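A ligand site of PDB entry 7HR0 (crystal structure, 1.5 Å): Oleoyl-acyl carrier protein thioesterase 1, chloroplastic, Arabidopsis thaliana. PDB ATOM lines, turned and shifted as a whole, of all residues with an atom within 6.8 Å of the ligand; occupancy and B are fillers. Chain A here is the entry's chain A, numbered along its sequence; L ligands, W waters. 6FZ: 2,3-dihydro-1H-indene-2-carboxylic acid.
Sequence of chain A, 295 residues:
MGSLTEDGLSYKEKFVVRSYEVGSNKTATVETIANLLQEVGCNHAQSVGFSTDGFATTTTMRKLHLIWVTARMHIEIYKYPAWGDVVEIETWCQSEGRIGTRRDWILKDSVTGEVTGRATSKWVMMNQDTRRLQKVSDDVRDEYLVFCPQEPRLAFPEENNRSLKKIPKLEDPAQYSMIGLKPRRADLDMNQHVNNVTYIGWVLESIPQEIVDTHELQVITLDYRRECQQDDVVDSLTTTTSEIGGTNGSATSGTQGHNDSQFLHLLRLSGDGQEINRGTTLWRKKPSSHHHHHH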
ATOM      1  N   ILE A  33      25.045 -22.347 -21.930  1.00  0.00           N
ATOM      2  CA  ILE A  33      25.582 -21.000 -22.246  1.00  0.00           C
ATOM      3  C   ILE A  33      25.910 -20.219 -20.983  1.00  0.00           C
ATOM      4  O   ILE A  33      27.033 -19.692 -20.846  1.00  0.00           O
ATOM      5  CB  ILE A  33      24.622 -20.197 -23.137  1.00  0.00           C
ATOM      6  CG1 ILE A  33      24.450 -20.906 -24.494  1.00  0.00           C
ATOM      7  CG2 ILE A  33      25.169 -18.735 -23.294  1.00  0.00           C
ATOM      8  CD1 ILE A  33      25.730 -21.043 -25.296  1.00  0.00           C
ATOM      9  N   ALA A  34      24.953 -20.205 -20.022  1.00  0.00           N
ATOM     10  CA  ALA A  34      25.164 -19.488 -18.770  1.00  0.00           C
ATOM     11  C   ALA A  34      26.399 -20.023 -18.000  1.00  0.00           C
ATOM     12  O   ALA A  34      27.152 -19.228 -17.405  1.00  0.00           O
ATOM     13  CB  ALA A  34      23.913 -19.582 -17.876  1.00  0.00           C
ATOM     14  N   ASN A  35      26.610 -21.362 -17.995  1.00  0.00           N
ATOM     15  CA  ASN A  35      27.779 -21.913 -17.300  1.00  0.00           C
ATOM     16  C   ASN A  35      29.080 -21.419 -18.013  1.00  0.00           C
ATOM     17  O   ASN A  35      30.050 -21.107 -17.322  1.00  0.00           O
ATOM     18  CB  ASN A  35      27.731 -23.427 -17.391  1.00  0.00           C
ATOM     19  CG  ASN A  35      26.892 -24.054 -16.293  1.00  0.00           C
ATOM     20  OD1 ASN A  35      26.844 -23.558 -15.176  1.00  0.00           O
ATOM     21  ND2 ASN A  35      26.248 -25.178 -16.578  1.00  0.00           N
ATOM     22  N   LEU A  37      29.448 -18.598 -19.655  1.00  0.00           N
ATOM     23  CA  LEU A  37      29.616 -17.183 -19.276  1.00  0.00           C
ATOM     24  C   LEU A  37      30.261 -17.094 -17.892  1.00  0.00           C
ATOM     25  O   LEU A  37      31.181 -16.321 -17.680  1.00  0.00           O
ATOM     26  CB  LEU A  37      28.255 -16.444 -19.276  1.00  0.00           C
ATOM     27  CG  LEU A  37      27.531 -16.435 -20.621  1.00  0.00           C
ATOM     28  CD1 LEU A  37      26.223 -15.650 -20.531  1.00  0.00           C
ATOM     29  CD2 LEU A  37      28.401 -15.879 -21.770  1.00  0.00           C
ATOM     30  N   GLN A  38      29.804 -17.939 -16.955  1.00  0.00           N
ATOM     31  CA  GLN A  38      30.381 -17.957 -15.610  1.00  0.00           C
ATOM     32  C   GLN A  38      31.867 -18.310 -15.627  1.00  0.00           C
ATOM     33  O   GLN A  38      32.700 -17.626 -15.008  1.00  0.00           O
ATOM     34  CB  GLN A  38      29.605 -18.945 -14.722  1.00  0.00           C
ATOM     35  CG  GLN A  38      29.944 -18.837 -13.272  1.00  0.00           C
ATOM     36  CD  GLN A  38      28.947 -19.704 -12.522  1.00  0.00           C
ATOM     37  OE1 GLN A  38      27.935 -19.205 -12.002  1.00  0.00           O
ATOM     38  NE2 GLN A  38      29.177 -21.015 -12.494  1.00  0.00           N
ATOM     39  N   GLU A  39      32.211 -19.380 -16.378  1.00  0.00           N
ATOM     40  CA  GLU A  39      33.592 -19.847 -16.503  1.00  0.00           C
ATOM     41  C   GLU A  39      34.524 -18.792 -17.095  1.00  0.00           C
ATOM     42  O   GLU A  39      35.566 -18.522 -16.488  1.00  0.00           O
ATOM     43  CB  GLU A  39      33.626 -21.155 -17.317  1.00  0.00           C
ATOM     44  CG  GLU A  39      35.036 -21.668 -17.628  1.00  0.00           C
ATOM     45  CD  GLU A  39      35.874 -22.104 -16.447  1.00  0.00           C
ATOM     46  OE1 GLU A  39      35.376 -22.016 -15.289  1.00  0.00           O
ATOM     47  OE2 GLU A  39      37.035 -22.516 -16.663  1.00  0.00           O
ATOM     48  N   GLY A  41      34.099 -15.616 -17.126  1.00  0.00           N
ATOM     49  CA  GLY A  41      34.152 -14.527 -16.157  1.00  0.00           C
ATOM     50  C   GLY A  41      35.137 -14.838 -15.045  1.00  0.00           C
ATOM     51  O   GLY A  41      35.962 -13.989 -14.684  1.00  0.00           O
ATOM     52  N   CYS A  42      35.100 -16.078 -14.525  1.00  0.00           N
ATOM     53  CA  CYS A  42      36.008 -16.521 -13.472  1.00  0.00           C
ATOM     54  C   CYS A  42      37.457 -16.543 -13.958  1.00  0.00           C
ATOM     55  O   CYS A  42      38.355 -16.111 -13.238  1.00  0.00           O
ATOM     56  CB  CYS A  42      35.602 -17.889 -12.932  1.00  0.00           C
ATOM     57  SG  CYS A  42      34.080 -17.879 -11.949  1.00  0.00           S
ATOM     58  N   THR A  70      25.285 -11.068  -7.468  1.00  0.00           N
ATOM     59  CA  THR A  70      24.554 -10.754  -8.690  1.00  0.00           C
ATOM     60  C   THR A  70      23.170 -10.191  -8.367  1.00  0.00           C
ATOM     61  O   THR A  70      22.449 -10.777  -7.554  1.00  0.00           O
ATOM     62  CB  THR A  70      24.351 -11.990  -9.590  1.00  0.00           C
ATOM     63  OG1 THR A  70      25.584 -12.701  -9.681  1.00  0.00           O
ATOM     64  CG2 THR A  70      23.885 -11.603 -10.975  1.00  0.00           C
ATOM     65  N   ARG A  72      21.208  -8.896 -11.257  1.00  0.00           N
ATOM     66  CA  ARG A  72      20.479  -9.215 -12.460  1.00  0.00           C
ATOM     67  C   ARG A  72      21.381  -9.876 -13.475  1.00  0.00           C
ATOM     68  O   ARG A  72      22.554  -9.482 -13.606  1.00  0.00           O
ATOM     69  CB  ARG A  72      19.874  -7.921 -13.090  1.00  0.00           C
ATOM     70  CG  ARG A  72      19.204  -8.141 -14.471  1.00  0.00           C
ATOM     71  CD  ARG A  72      18.471  -6.925 -15.032  1.00  0.00           C
ATOM     72  NE  ARG A  72      17.206  -6.734 -14.332  1.00  0.00           N
ATOM     73  CZ  ARG A  72      16.205  -5.968 -14.749  1.00  0.00           C
ATOM     74  NH1 ARG A  72      16.309  -5.296 -15.895  1.00  0.00           N
ATOM     75  NH2 ARG A  72      15.100  -5.867 -14.030  1.00  0.00           N
ATOM     76  N   MET A  73      20.803 -10.822 -14.249  1.00  0.00           N
ATOM     77  CA  MET A  73      21.444 -11.425 -15.416  1.00  0.00           C
ATOM     78  C   MET A  73      20.496 -11.251 -16.625  1.00  0.00           C
ATOM     79  O   MET A  73      19.285 -11.469 -16.503  1.00  0.00           O
ATOM     80  CB  MET A  73      21.771 -12.910 -15.141  1.00  0.00           C
ATOM     81  CG  MET A  73      22.431 -13.604 -16.330  1.00  0.00           C
ATOM     82  SD  MET A  73      24.018 -12.782 -16.776  1.00  0.00           S
ATOM     83  CE  MET A  73      24.864 -14.088 -17.569  1.00  0.00           C
ATOM     84  N   ILE A  75      20.404 -12.286 -20.803  1.00  0.00           N
ATOM     85  CA  ILE A  75      21.053 -12.995 -21.911  1.00  0.00           C
ATOM     86  C   ILE A  75      20.171 -12.943 -23.159  1.00  0.00           C
ATOM     87  O   ILE A  75      18.961 -13.162 -23.048  1.00  0.00           O
ATOM     88  CB  ILE A  75      21.277 -14.484 -21.535  1.00  0.00           C
ATOM     89  CG1 ILE A  75      22.025 -14.627 -20.228  1.00  0.00           C
ATOM     90  CG2 ILE A  75      21.974 -15.249 -22.701  1.00  0.00           C
ATOM     91  CD1 ILE A  75      22.082 -16.040 -19.708  1.00  0.00           C
ATOM     92  N   ARG A 103      29.352  -6.891 -15.519  1.00  0.00           N
ATOM     93  CA  ARG A 103      30.205  -7.729 -16.340  1.00  0.00           C
ATOM     94  C   ARG A 103      29.371  -7.979 -17.600  1.00  0.00           C
ATOM     95  O   ARG A 103      28.225  -8.411 -17.493  1.00  0.00           O
ATOM     96  CB  ARG A 103      30.580  -9.084 -15.694  1.00  0.00           C
ATOM     97  CG  ARG A 103      31.330  -9.969 -16.677  1.00  0.00           C
ATOM     98  CD  ARG A 103      31.912 -11.218 -16.054  1.00  0.00           C
ATOM     99  NE  ARG A 103      33.024 -10.956 -15.144  1.00  0.00           N
ATOM    100  CZ  ARG A 103      34.274 -10.711 -15.556  1.00  0.00           C
ATOM    101  NH1 ARG A 103      35.247 -10.500 -14.673  1.00  0.00           N
ATOM    102  NH2 ARG A 103      34.543 -10.607 -16.858  1.00  0.00           N
ATOM    103  N   TRP A 105      29.266  -9.687 -21.791  1.00  0.00           N
ATOM    104  CA  TRP A 105      29.843 -10.718 -22.649  1.00  0.00           C
ATOM    105  C   TRP A 105      29.321 -10.622 -24.068  1.00  0.00           C
ATOM    106  O   TRP A 105      28.141 -10.296 -24.271  1.00  0.00           O
ATOM    107  CB  TRP A 105      29.429 -12.127 -22.169  1.00  0.00           C
ATOM    108  CG  TRP A 105      29.853 -12.556 -20.781  1.00  0.00           C
ATOM    109  CD1 TRP A 105      30.823 -13.468 -20.475  1.00  0.00           C
ATOM    110  CD2 TRP A 105      29.102 -12.331 -19.563  1.00  0.00           C
ATOM    111  NE1 TRP A 105      30.793 -13.749 -19.101  1.00  0.00           N
ATOM    112  CE2 TRP A 105      29.725 -13.084 -18.542  1.00  0.00           C
ATOM    113  CE3 TRP A 105      27.989 -11.548 -19.225  1.00  0.00           C
ATOM    114  CZ2 TRP A 105      29.261 -13.082 -17.217  1.00  0.00           C
ATOM    115  CZ3 TRP A 105      27.527 -11.537 -17.922  1.00  0.00           C
ATOM    116  CH2 TRP A 105      28.139 -12.338 -16.931  1.00  0.00           C
ATOM    117  N   SER A 121      25.417  -8.468 -16.884  1.00  0.00           N
ATOM    118  CA  SER A 121      25.065  -8.750 -15.488  1.00  0.00           C
ATOM    119  C   SER A 121      25.355  -7.536 -14.619  1.00  0.00           C
ATOM    120  O   SER A 121      26.340  -6.812 -14.882  1.00  0.00           O
ATOM    121  CB  SER A 121      25.811  -9.993 -15.005  1.00  0.00           C
ATOM    122  OG  SER A 121      27.216  -9.806 -15.041  1.00  0.00           O
ATOM    123  N   TRP A 123      26.049  -6.275 -10.602  1.00  0.00           N
ATOM    124  CA  TRP A 123      26.550  -6.789  -9.314  1.00  0.00           C
ATOM    125  C   TRP A 123      26.500  -5.679  -8.287  1.00  0.00           C
ATOM    126  O   TRP A 123      26.737  -4.505  -8.595  1.00  0.00           O
ATOM    127  CB  TRP A 123      28.009  -7.266  -9.442  1.00  0.00           C
ATOM    128  CG  TRP A 123      28.180  -8.372 -10.444  1.00  0.00           C
ATOM    129  CD1 TRP A 123      28.157  -8.248 -11.799  1.00  0.00           C
ATOM    130  CD2 TRP A 123      28.347  -9.776 -10.178  1.00  0.00           C
ATOM    131  NE1 TRP A 123      28.306  -9.479 -12.398  1.00  0.00           N
ATOM    132  CE2 TRP A 123      28.477 -10.431 -11.421  1.00  0.00           C
ATOM    133  CE3 TRP A 123      28.475 -10.529  -9.008  1.00  0.00           C
ATOM    134  CZ2 TRP A 123      28.603 -11.807 -11.525  1.00  0.00           C
ATOM    135  CZ3 TRP A 123      28.694 -11.891  -9.122  1.00  0.00           C
ATOM    136  CH2 TRP A 123      28.771 -12.509 -10.369  1.00  0.00           C
ATOM    137  N   ASN A 195      24.328 -22.376  -7.131  1.00  0.00           N
ATOM    138  CA  ASN A 195      24.927 -21.718  -8.293  1.00  0.00           C
ATOM    139  C   ASN A 195      23.891 -20.837  -8.970  1.00  0.00           C
ATOM    140  O   ASN A 195      22.725 -21.251  -9.113  1.00  0.00           O
ATOM    141  CB  ASN A 195      25.435 -22.793  -9.275  1.00  0.00           C
ATOM    142  CG  ASN A 195      26.309 -22.187 -10.354  1.00  0.00           C
ATOM    143  OD1 ASN A 195      25.841 -21.379 -11.171  1.00  0.00           O
ATOM    144  ND2 ASN A 195      27.610 -22.504 -10.352  1.00  0.00           N
ATOM    145  N   ASN A 196      24.291 -19.648  -9.429  1.00  0.00           N
ATOM    146  CA  ASN A 196      23.365 -18.748 -10.103  1.00  0.00           C
ATOM    147  C   ASN A 196      22.640 -19.387 -11.286  1.00  0.00           C
ATOM    148  O   ASN A 196      21.518 -18.997 -11.603  1.00  0.00           O
ATOM    149  CB  ASN A 196      24.142 -17.543 -10.666  1.00  0.00           C
ATOM    150  CG  ASN A 196      24.486 -16.506  -9.652  1.00  0.00           C
ATOM    151  OD1 ASN A 196      23.903 -16.457  -8.541  1.00  0.00           O
ATOM    152  ND2 ASN A 196      25.449 -15.625 -10.032  1.00  0.00           N
ATOM    153  N   VAL A 197      23.327 -20.309 -12.003  1.00  0.00           N
ATOM    154  CA  VAL A 197      22.710 -20.919 -13.185  1.00  0.00           C
ATOM    155  C   VAL A 197      21.506 -21.820 -12.784  1.00  0.00           C
ATOM    156  O   VAL A 197      20.565 -21.990 -13.571  1.00  0.00           O
ATOM    157  CB  VAL A 197      23.745 -21.746 -13.977  1.00  0.00           C
ATOM    158  CG1 VAL A 197      23.088 -22.398 -15.165  1.00  0.00           C
ATOM    159  CG2 VAL A 197      24.923 -20.854 -14.393  1.00  0.00           C
ATOM    160  N   THR A 198      21.537 -22.395 -11.553  1.00  0.00           N
ATOM    161  CA  THR A 198      20.451 -23.282 -11.128  1.00  0.00           C
ATOM    162  C   THR A 198      19.102 -22.573 -11.145  1.00  0.00           C
ATOM    163  O   THR A 198      18.093 -23.164 -11.551  1.00  0.00           O
ATOM    164  CB  THR A 198      20.751 -23.846  -9.717  1.00  0.00           C
ATOM    165  OG1 THR A 198      21.941 -24.653  -9.821  1.00  0.00           O
ATOM    166  CG2 THR A 198      19.608 -24.716  -9.192  1.00  0.00           C
ATOM    167  N   ILE A 200      18.112 -20.192 -13.154  1.00  0.00           N
ATOM    168  CA  ILE A 200      17.606 -20.139 -14.537  1.00  0.00           C
ATOM    169  C   ILE A 200      16.850 -21.466 -14.864  1.00  0.00           C
ATOM    170  O   ILE A 200      15.725 -21.462 -15.353  1.00  0.00           O
ATOM    171  CB  ILE A 200      18.787 -19.960 -15.524  1.00  0.00           C
ATOM    172  CG1 ILE A 200      19.374 -18.581 -15.329  1.00  0.00           C
ATOM    173  CG2 ILE A 200      18.290 -20.184 -16.970  1.00  0.00           C
ATOM    174  CD1 ILE A 200      20.609 -18.251 -16.220  1.00  0.00           C
ATOM    175  N   LEU A 222      16.637 -11.915 -15.591  1.00  0.00           N
ATOM    176  CA  LEU A 222      16.338 -12.474 -14.268  1.00  0.00           C
ATOM    177  C   LEU A 222      16.897 -11.626 -13.144  1.00  0.00           C
ATOM    178  O   LEU A 222      18.106 -11.409 -13.092  1.00  0.00           O
ATOM    179  CB  LEU A 222      16.948 -13.908 -14.212  1.00  0.00           C
ATOM    180  CG  LEU A 222      16.531 -14.835 -13.087  1.00  0.00           C
ATOM    181  CD1 LEU A 222      14.999 -14.917 -12.940  1.00  0.00           C
ATOM    182  CD2 LEU A 222      17.067 -16.251 -13.325  1.00  0.00           C
ATOM    183  N   TYR A 224      17.668 -11.294  -9.053  1.00  0.00           N
ATOM    184  CA  TYR A 224      18.019 -12.137  -7.911  1.00  0.00           C
ATOM    185  C   TYR A 224      17.747 -11.308  -6.638  1.00  0.00           C
ATOM    186  O   TYR A 224      18.362 -10.252  -6.427  1.00  0.00           O
ATOM    187  CB  TYR A 224      19.531 -12.510  -7.983  1.00  0.00           C
ATOM    188  CG  TYR A 224      19.831 -13.538  -9.054  1.00  0.00           C
ATOM    189  CD1 TYR A 224      19.874 -13.176 -10.399  1.00  0.00           C
ATOM    190  CD2 TYR A 224      20.166 -14.845  -8.707  1.00  0.00           C
ATOM    191  CE1 TYR A 224      20.102 -14.128 -11.378  1.00  0.00           C
ATOM    192  CE2 TYR A 224      20.398 -15.807  -9.694  1.00  0.00           C
ATOM    193  CZ  TYR A 224      20.404 -15.433 -11.027  1.00  0.00           C
ATOM    194  OH  TYR A 224      20.653 -16.390 -12.001  1.00  0.00           O
HETATM  195  C1  6FZ L   1      23.804 -17.178 -14.871  1.00  0.00           C
HETATM  196  C2  6FZ L   1      25.117 -16.976 -15.267  1.00  0.00           C
HETATM  197  C3  6FZ L   1      25.856 -15.964 -14.658  1.00  0.00           C
HETATM  198  C4  6FZ L   1      25.258 -15.101 -13.764  1.00  0.00           C
HETATM  199  C5  6FZ L   1      23.922 -15.262 -13.416  1.00  0.00           C
HETATM  200  C6  6FZ L   1      26.225 -14.036 -13.313  1.00  0.00           C
HETATM  201  C7  6FZ L   1      27.598 -14.577 -13.774  1.00  0.00           C
HETATM  202  C8  6FZ L   1      27.256 -15.500 -14.969  1.00  0.00           C
HETATM  203  O1  6FZ L   1      27.595 -15.970 -11.905  1.00  0.00           O
HETATM  204  C9  6FZ L   1      28.337 -15.387 -12.714  1.00  0.00           C
HETATM  205  O   6FZ L   1      29.554 -15.441 -12.674  1.00  0.00           O
HETATM  206  C   6FZ L   1      23.203 -16.305 -13.978  1.00  0.00           C
HETATM  207  O   HOH W   1      28.511 -16.559  -9.387  1.00  0.00           O
HETATM  208  O   HOH W   2      31.623 -14.859 -14.027  1.00  0.00           O
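OE1 of Gln 38 lies close to O1 of the ligand. ND2 of Asn 196 lies within hydrogen-bond range of O1 of the ligand, at 2.9 Å.
The backbone carbonyl oxygen (O) of Gln 38 sits at hydrogen-bond distance from the side-chain sulfur (SG) of Cys 42. The indole nitrogen (NE1) of Trp 123 lies within hydrogen-bond range of the side-chain hydroxyl (OG) of Ser 121. The backbone carbonyl oxygen (O) of Asn 196 is in hydrogen-bond range of the side-chain hydroxyl (OH) of Tyr 224, at 2.8 Å. ND2 of Asn 196 sits at hydrogen-bond distance from OG1 of Thr 70, at 2.9 Å. NE1 of Trp 105 lies within hydrogen-bond range of O of Leu 37 (3.0 Å). ND2 of Asn 195 lies close to NE2 of Gln 38, at 3.0 Å. The backbone NH of Val 197 is in hydrogen-bond range of the side-chain amide oxygen of Asn 195 (2.9 Å). O of Met 73 is in hydrogen-bond range of N of Leu 222.
Ala 34 touches the ligand. OG1 of Thr 70 touches C6 of the ligand (3.9 Å). CE of Met 73 touches C3 of the ligand, 3.6 Å away. Trp 105 touches the ligand (CH2 to C8, 3.8 Å). Trp 123 touches the ligand. Val 197 touches the ligand. Ile 200 touches the ligand. OH of Tyr 224 touches C of the ligand, 3.2 Å away. Hydrophobic or aromatic side chains within 4 Å of the ligand: Ala 34, Met 73, Trp 105, Trp 123, Val 197 and Ile 200. Within 4 Å of the ligand: Ala 34, Gln 38, Thr 70, Met 73, Trp 105, Trp 123, Asn 196, Val 197, Ile 200 and Tyr 224.
Water W2 bridges an oxygen (O) of the ligand and the backbone carbonyl oxygen of Gln 38. Water W1 bridges O1 of the ligand and ND2 of Asn 196.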
